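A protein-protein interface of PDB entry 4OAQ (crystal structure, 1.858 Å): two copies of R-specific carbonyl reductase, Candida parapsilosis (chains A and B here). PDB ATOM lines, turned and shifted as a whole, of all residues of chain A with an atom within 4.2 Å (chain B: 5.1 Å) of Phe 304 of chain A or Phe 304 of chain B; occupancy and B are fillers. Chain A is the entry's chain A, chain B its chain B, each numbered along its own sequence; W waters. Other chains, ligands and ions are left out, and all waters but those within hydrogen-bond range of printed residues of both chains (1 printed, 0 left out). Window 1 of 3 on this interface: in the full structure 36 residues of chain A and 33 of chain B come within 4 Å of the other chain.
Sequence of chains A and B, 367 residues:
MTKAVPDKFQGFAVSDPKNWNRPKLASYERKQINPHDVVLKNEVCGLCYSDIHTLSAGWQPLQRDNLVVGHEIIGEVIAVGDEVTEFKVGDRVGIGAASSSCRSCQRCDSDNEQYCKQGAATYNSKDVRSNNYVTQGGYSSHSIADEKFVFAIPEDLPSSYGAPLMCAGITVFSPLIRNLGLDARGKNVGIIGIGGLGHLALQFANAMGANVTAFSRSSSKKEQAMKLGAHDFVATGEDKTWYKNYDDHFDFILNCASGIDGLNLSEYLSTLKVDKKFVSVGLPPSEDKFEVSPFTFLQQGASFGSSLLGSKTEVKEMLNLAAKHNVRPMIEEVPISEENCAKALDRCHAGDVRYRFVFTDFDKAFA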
ATOM      1  N   LEU A 265     -12.884  -7.880   2.907  1.00  0.00           N
ATOM      2  CA  LEU A 265     -13.214  -6.919   3.956  1.00  0.00           C
ATOM      3  C   LEU A 265     -14.516  -7.255   4.680  1.00  0.00           C
ATOM      4  O   LEU A 265     -14.581  -7.105   5.895  1.00  0.00           O
ATOM      5  CB  LEU A 265     -13.247  -5.491   3.398  1.00  0.00           C
ATOM      6  CG  LEU A 265     -13.587  -4.401   4.409  1.00  0.00           C
ATOM      7  CD1 LEU A 265     -12.603  -4.421   5.550  1.00  0.00           C
ATOM      8  CD2 LEU A 265     -13.585  -3.048   3.727  1.00  0.00           C
ATOM      9  N   PHE A 278     -12.646  -1.228  11.946  1.00  0.00           N
ATOM     10  CA  PHE A 278     -11.630  -1.817  11.099  1.00  0.00           C
ATOM     11  C   PHE A 278     -10.803  -0.628  10.627  1.00  0.00           C
ATOM     12  O   PHE A 278     -11.356   0.328  10.052  1.00  0.00           O
ATOM     13  CB  PHE A 278     -12.271  -2.542   9.903  1.00  0.00           C
ATOM     14  CG  PHE A 278     -11.280  -3.284   9.015  1.00  0.00           C
ATOM     15  CD1 PHE A 278     -11.224  -4.674   9.028  1.00  0.00           C
ATOM     16  CD2 PHE A 278     -10.431  -2.595   8.158  1.00  0.00           C
ATOM     17  CE1 PHE A 278     -10.328  -5.377   8.213  1.00  0.00           C
ATOM     18  CE2 PHE A 278      -9.520  -3.279   7.341  1.00  0.00           C
ATOM     19  CZ  PHE A 278      -9.478  -4.686   7.358  1.00  0.00           C
ATOM     20  N   PHE A 290     -11.065  -2.183  -1.656  1.00  0.00           N
ATOM     21  CA  PHE A 290     -11.844  -3.201  -0.978  1.00  0.00           C
ATOM     22  C   PHE A 290     -13.311  -3.061  -1.403  1.00  0.00           C
ATOM     23  O   PHE A 290     -13.734  -1.985  -1.820  1.00  0.00           O
ATOM     24  CB  PHE A 290     -11.703  -3.028   0.531  1.00  0.00           C
ATOM     25  CG  PHE A 290     -10.276  -3.060   1.013  1.00  0.00           C
ATOM     26  CD1 PHE A 290      -9.538  -4.238   0.962  1.00  0.00           C
ATOM     27  CD2 PHE A 290      -9.673  -1.919   1.530  1.00  0.00           C
ATOM     28  CE1 PHE A 290      -8.224  -4.270   1.412  1.00  0.00           C
ATOM     29  CE2 PHE A 290      -8.351  -1.954   1.975  1.00  0.00           C
ATOM     30  CZ  PHE A 290      -7.632  -3.133   1.913  1.00  0.00           C
ATOM     31  N   PHE A 297     -22.201  -3.649   6.755  1.00  0.00           N
ATOM     32  CA  PHE A 297     -21.990  -2.534   7.680  1.00  0.00           C
ATOM     33  C   PHE A 297     -23.140  -2.527   8.674  1.00  0.00           C
ATOM     34  O   PHE A 297     -22.939  -2.341   9.869  1.00  0.00           O
ATOM     35  CB  PHE A 297     -21.963  -1.185   6.960  1.00  0.00           C
ATOM     36  CG  PHE A 297     -20.640  -0.832   6.376  1.00  0.00           C
ATOM     37  CD1 PHE A 297     -19.546  -0.616   7.191  1.00  0.00           C
ATOM     38  CD2 PHE A 297     -20.498  -0.680   5.007  1.00  0.00           C
ATOM     39  CE1 PHE A 297     -18.318  -0.283   6.643  1.00  0.00           C
ATOM     40  CE2 PHE A 297     -19.281  -0.351   4.454  1.00  0.00           C
ATOM     41  CZ  PHE A 297     -18.186  -0.152   5.274  1.00  0.00           C
ATOM     42  N   SER A 303     -17.395   0.092  11.486  1.00  0.00           N
ATOM     43  CA  SER A 303     -16.888   1.182  10.665  1.00  0.00           C
ATOM     44  C   SER A 303     -15.634   0.741   9.941  1.00  0.00           C
ATOM     45  O   SER A 303     -14.917  -0.137  10.410  1.00  0.00           O
ATOM     46  CB  SER A 303     -16.589   2.401  11.533  1.00  0.00           C
ATOM     47  OG  SER A 303     -15.627   2.073  12.515  1.00  0.00           O
ATOM     48  N   PHE A 304     -15.382   1.348   8.788  1.00  0.00           N
ATOM     49  CA  PHE A 304     -14.128   1.182   8.090  1.00  0.00           C
ATOM     50  C   PHE A 304     -13.413   2.530   8.047  1.00  0.00           C
ATOM     51  O   PHE A 304     -14.047   3.566   7.824  1.00  0.00           O
ATOM     52  CB  PHE A 304     -14.360   0.669   6.665  1.00  0.00           C
ATOM     53  CG  PHE A 304     -13.116   0.645   5.831  1.00  0.00           C
ATOM     54  CD1 PHE A 304     -12.292  -0.475   5.829  1.00  0.00           C
ATOM     55  CD2 PHE A 304     -12.760   1.739   5.051  1.00  0.00           C
ATOM     56  CE1 PHE A 304     -11.140  -0.507   5.067  1.00  0.00           C
ATOM     57  CE2 PHE A 304     -11.589   1.720   4.277  1.00  0.00           C
ATOM     58  CZ  PHE A 304     -10.782   0.587   4.286  1.00  0.00           C
ATOM     59  N   GLY A 305     -12.096   2.509   8.226  1.00  0.00           N
ATOM     60  CA  GLY A 305     -11.298   3.724   8.223  1.00  0.00           C
ATOM     61  C   GLY A 305      -9.812   3.467   8.029  1.00  0.00           C
ATOM     62  O   GLY A 305      -9.401   2.335   7.809  1.00  0.00           O
ATOM     63  N   ILE B 260     -25.724   7.978  -0.921  1.00  0.00           N
ATOM     64  CA  ILE B 260     -24.269   7.980  -0.817  1.00  0.00           C
ATOM     65  C   ILE B 260     -23.587   8.232  -2.168  1.00  0.00           C
ATOM     66  O   ILE B 260     -22.535   8.872  -2.225  1.00  0.00           O
ATOM     67  CB  ILE B 260     -23.745   6.681  -0.125  1.00  0.00           C
ATOM     68  CG1 ILE B 260     -22.483   6.973   0.695  1.00  0.00           C
ATOM     69  CG2 ILE B 260     -23.535   5.542  -1.127  1.00  0.00           C
ATOM     70  CD1 ILE B 260     -22.644   6.684   2.177  1.00  0.00           C
ATOM     71  N   LEU B 265     -18.492  12.218  -0.755  1.00  0.00           N
ATOM     72  CA  LEU B 265     -18.005  11.819   0.555  1.00  0.00           C
ATOM     73  C   LEU B 265     -16.724  12.545   0.932  1.00  0.00           C
ATOM     74  O   LEU B 265     -16.547  12.932   2.091  1.00  0.00           O
ATOM     75  CB  LEU B 265     -17.766  10.312   0.573  1.00  0.00           C
ATOM     76  CG  LEU B 265     -17.415   9.685   1.917  1.00  0.00           C
ATOM     77  CD1 LEU B 265     -18.521   9.942   2.933  1.00  0.00           C
ATOM     78  CD2 LEU B 265     -17.181   8.194   1.740  1.00  0.00           C
ATOM     79  N   PHE B 278     -18.101   9.385   9.899  1.00  0.00           N
ATOM     80  CA  PHE B 278     -19.216   9.747   9.035  1.00  0.00           C
ATOM     81  C   PHE B 278     -20.120   8.534   9.099  1.00  0.00           C
ATOM     82  O   PHE B 278     -19.723   7.460   8.687  1.00  0.00           O
ATOM     83  CB  PHE B 278     -18.706   9.946   7.605  1.00  0.00           C
ATOM     84  CG  PHE B 278     -19.764  10.333   6.606  1.00  0.00           C
ATOM     85  CD1 PHE B 278     -19.861  11.645   6.156  1.00  0.00           C
ATOM     86  CD2 PHE B 278     -20.617   9.385   6.060  1.00  0.00           C
ATOM     87  CE1 PHE B 278     -20.816  12.006   5.214  1.00  0.00           C
ATOM     88  CE2 PHE B 278     -21.572   9.752   5.097  1.00  0.00           C
ATOM     89  CZ  PHE B 278     -21.662  11.069   4.685  1.00  0.00           C
ATOM     90  N   VAL B 292     -14.375   0.693  -1.464  1.00  0.00           N
ATOM     91  CA  VAL B 292     -13.869   1.621  -0.455  1.00  0.00           C
ATOM     92  C   VAL B 292     -12.342   1.636  -0.512  1.00  0.00           C
ATOM     93  O   VAL B 292     -11.703   0.603  -0.755  1.00  0.00           O
ATOM     94  CB  VAL B 292     -14.409   1.301   0.970  1.00  0.00           C
ATOM     95  CG1 VAL B 292     -13.833   0.000   1.505  1.00  0.00           C
ATOM     96  CG2 VAL B 292     -14.129   2.438   1.915  1.00  0.00           C
ATOM     97  N   SER B 293     -11.769   2.821  -0.338  1.00  0.00           N
ATOM     98  CA  SER B 293     -10.325   2.992  -0.375  1.00  0.00           C
ATOM     99  C   SER B 293      -9.843   3.656   0.913  1.00  0.00           C
ATOM    100  O   SER B 293     -10.463   4.593   1.391  1.00  0.00           O
ATOM    101  CB  SER B 293      -9.927   3.861  -1.564  1.00  0.00           C
ATOM    102  OG  SER B 293      -8.659   4.464  -1.329  1.00  0.00           O
ATOM    103  N   PRO B 294      -8.734   3.169   1.478  1.00  0.00           N
ATOM    104  CA  PRO B 294      -8.194   3.767   2.711  1.00  0.00           C
ATOM    105  C   PRO B 294      -7.770   5.225   2.515  1.00  0.00           C
ATOM    106  O   PRO B 294      -7.801   6.043   3.455  1.00  0.00           O
ATOM    107  CB  PRO B 294      -6.974   2.878   3.031  1.00  0.00           C
ATOM    108  CG  PRO B 294      -6.636   2.192   1.746  1.00  0.00           C
ATOM    109  CD  PRO B 294      -7.950   2.007   1.029  1.00  0.00           C
ATOM    110  N   PHE B 297      -9.886   8.153   3.575  1.00  0.00           N
ATOM    111  CA  PHE B 297      -9.990   8.497   4.994  1.00  0.00           C
ATOM    112  C   PHE B 297      -8.664   8.911   5.597  1.00  0.00           C
ATOM    113  O   PHE B 297      -8.639   9.500   6.670  1.00  0.00           O
ATOM    114  CB  PHE B 297     -10.549   7.302   5.767  1.00  0.00           C
ATOM    115  CG  PHE B 297     -11.840   6.786   5.202  1.00  0.00           C
ATOM    116  CD1 PHE B 297     -13.055   7.347   5.574  1.00  0.00           C
ATOM    117  CD2 PHE B 297     -11.834   5.754   4.275  1.00  0.00           C
ATOM    118  CE1 PHE B 297     -14.255   6.868   5.025  1.00  0.00           C
ATOM    119  CE2 PHE B 297     -13.017   5.275   3.737  1.00  0.00           C
ATOM    120  CZ  PHE B 297     -14.223   5.837   4.105  1.00  0.00           C
ATOM    121  N   ALA B 302     -10.121   9.250   9.463  1.00  0.00           N
ATOM    122  CA  ALA B 302     -11.576   9.143   9.551  1.00  0.00           C
ATOM    123  C   ALA B 302     -12.065   7.716   9.393  1.00  0.00           C
ATOM    124  O   ALA B 302     -11.313   6.815   8.993  1.00  0.00           O
ATOM    125  CB  ALA B 302     -12.212  10.014   8.477  1.00  0.00           C
ATOM    126  N   SER B 303     -13.347   7.533   9.679  1.00  0.00           N
ATOM    127  CA  SER B 303     -14.012   6.261   9.467  1.00  0.00           C
ATOM    128  C   SER B 303     -15.396   6.479   8.874  1.00  0.00           C
ATOM    129  O   SER B 303     -15.979   7.564   8.985  1.00  0.00           O
ATOM    130  CB  SER B 303     -14.115   5.470  10.771  1.00  0.00           C
ATOM    131  OG  SER B 303     -12.839   5.054  11.216  1.00  0.00           O
ATOM    132  N   PHE B 304     -15.900   5.430   8.235  1.00  0.00           N
ATOM    133  CA  PHE B 304     -17.202   5.425   7.608  1.00  0.00           C
ATOM    134  C   PHE B 304     -17.928   4.210   8.151  1.00  0.00           C
ATOM    135  O   PHE B 304     -17.335   3.137   8.275  1.00  0.00           O
ATOM    136  CB  PHE B 304     -17.037   5.242   6.092  1.00  0.00           C
ATOM    137  CG  PHE B 304     -18.322   5.338   5.322  1.00  0.00           C
ATOM    138  CD1 PHE B 304     -19.099   6.478   5.385  1.00  0.00           C
ATOM    139  CD2 PHE B 304     -18.757   4.298   4.522  1.00  0.00           C
ATOM    140  N   GLY B 305     -19.215   4.353   8.443  1.00  0.00           N
ATOM    141  CA  GLY B 305     -20.009   3.182   8.774  1.00  0.00           C
ATOM    142  C   GLY B 305     -21.495   3.449   8.853  1.00  0.00           C
ATOM    143  O   GLY B 305     -21.991   4.476   8.370  1.00  0.00           O
ATOM    144  N   SER B 306     -22.211   2.508   9.465  1.00  0.00           N
ATOM    145  CA  SER B 306     -23.658   2.578   9.559  1.00  0.00           C
ATOM    146  C   SER B 306     -24.136   2.447  10.994  1.00  0.00           C
ATOM    147  O   SER B 306     -23.367   2.115  11.896  1.00  0.00           O
ATOM    148  CB  SER B 306     -24.302   1.462   8.737  1.00  0.00           C
ATOM    149  OG  SER B 306     -24.405   1.829   7.376  1.00  0.00           O
HETATM  150  O   HOH W   1     -13.141   2.381  11.502  1.00  0.00           O
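Printed residues of chain B that touch a printed residue of chain A: Val 292, Phe 297, Ala 302, Ser 303, Phe 304 and Ser 306.
Hydrophobic or aromatic side chains of chain B within 4 Å of the printed part of chain A: Val 292, Phe 297 and Phe 304.
The backbone carbonyl oxygen of Phe 304 of chain A sits at hydrogen-bond distance from the backbone NH of Phe 304 of chain B.
O of Phe 290 of chain A is in hydrogen-bond range of N of Val 292 of chain B (2.8 Å).
Water W1 lies within hydrogen-bond range of OG of Ser 303 of chain A, OG of Ser 303 of chain B, O of Phe 278 of chain A and N of Gly 305 of chain A.
O of Phe 278 of chain A is in hydrogen-bond range of N of Gly 305 of chain A (2.9 Å).
O of Ser 303 of chain B sits at hydrogen-bond distance from N of Phe 278 of chain B, at 2.9 Å.
O of Ser 303 of chain A sits at hydrogen-bond distance from N of Phe 278 of chain A, at 3.0 Å.
O of Phe 297 of chain B is in hydrogen-bond range of N of Ala 302 of chain B, 3.2 Å away.
Phe 297 of chain A touches Phe 304 of chain B, and with the chains exchanged Phe 304 of chain A touches Phe 297 of chain B.
Ser 303 of chain A touches Phe 304 of chain B, and with the chains exchanged Phe 304 of chain A touches Ser 303 of chain B.
Phe 304 of chain A touches its own counterpart, Phe 304 of chain B.
Gly 305 of chain A touches Ser 303 of chain B, but with the chains exchanged Ser 303 of chain A does not touch Gly 305 of chain B (4.2 Å).
Positions printed for both chains: 265, 278, 297, 303, 304 and 305.
Of chain B, only Val 292, Phe 297, Ser 303 and Phe 304 come within 4 Å of Phe 304 of chain A.
Of chain A, only Phe 297 (3.9 Å), Ser 303 (3.1 Å) and Phe 304 (2.7 Å) come within 4 Å of Phe 304 of chain B.
Printed residues of chain B within 4 Å of Ser 303 of chain A: Phe 304 (3.1 Å).
Of the printed residues of chain A, Val 292 of chain B touches Leu 265 (3.8 Å), Phe 290 (2.8 Å) and Phe 304 (3.5 Å).
Of the printed residues of chain B, Leu 265 of chain A touches Val 292.
The nearest printed residue of chain B that does not touch Phe 304 of chain A is Ser 293 of chain B (4.2 Å).
Among the printed residues, pairs that only touch across the chains: Leu 265 of chain A with Val 292 of chain B, Phe 297 of chain A with Phe 304 of chain B, Phe 297 of chain A with Ser 306 of chain B, Ser 303 of chain A with Phe 304 of chain B, Phe 304 of chain A with Val 292 of chain B, Phe 304 of chain A with Phe 297 of chain B, Phe 304 of chain A with Ser 303 of chain B, Gly 305 of chain A with Ala 302 of chain B and Gly 305 of chain A with Ser 303 of chain B.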
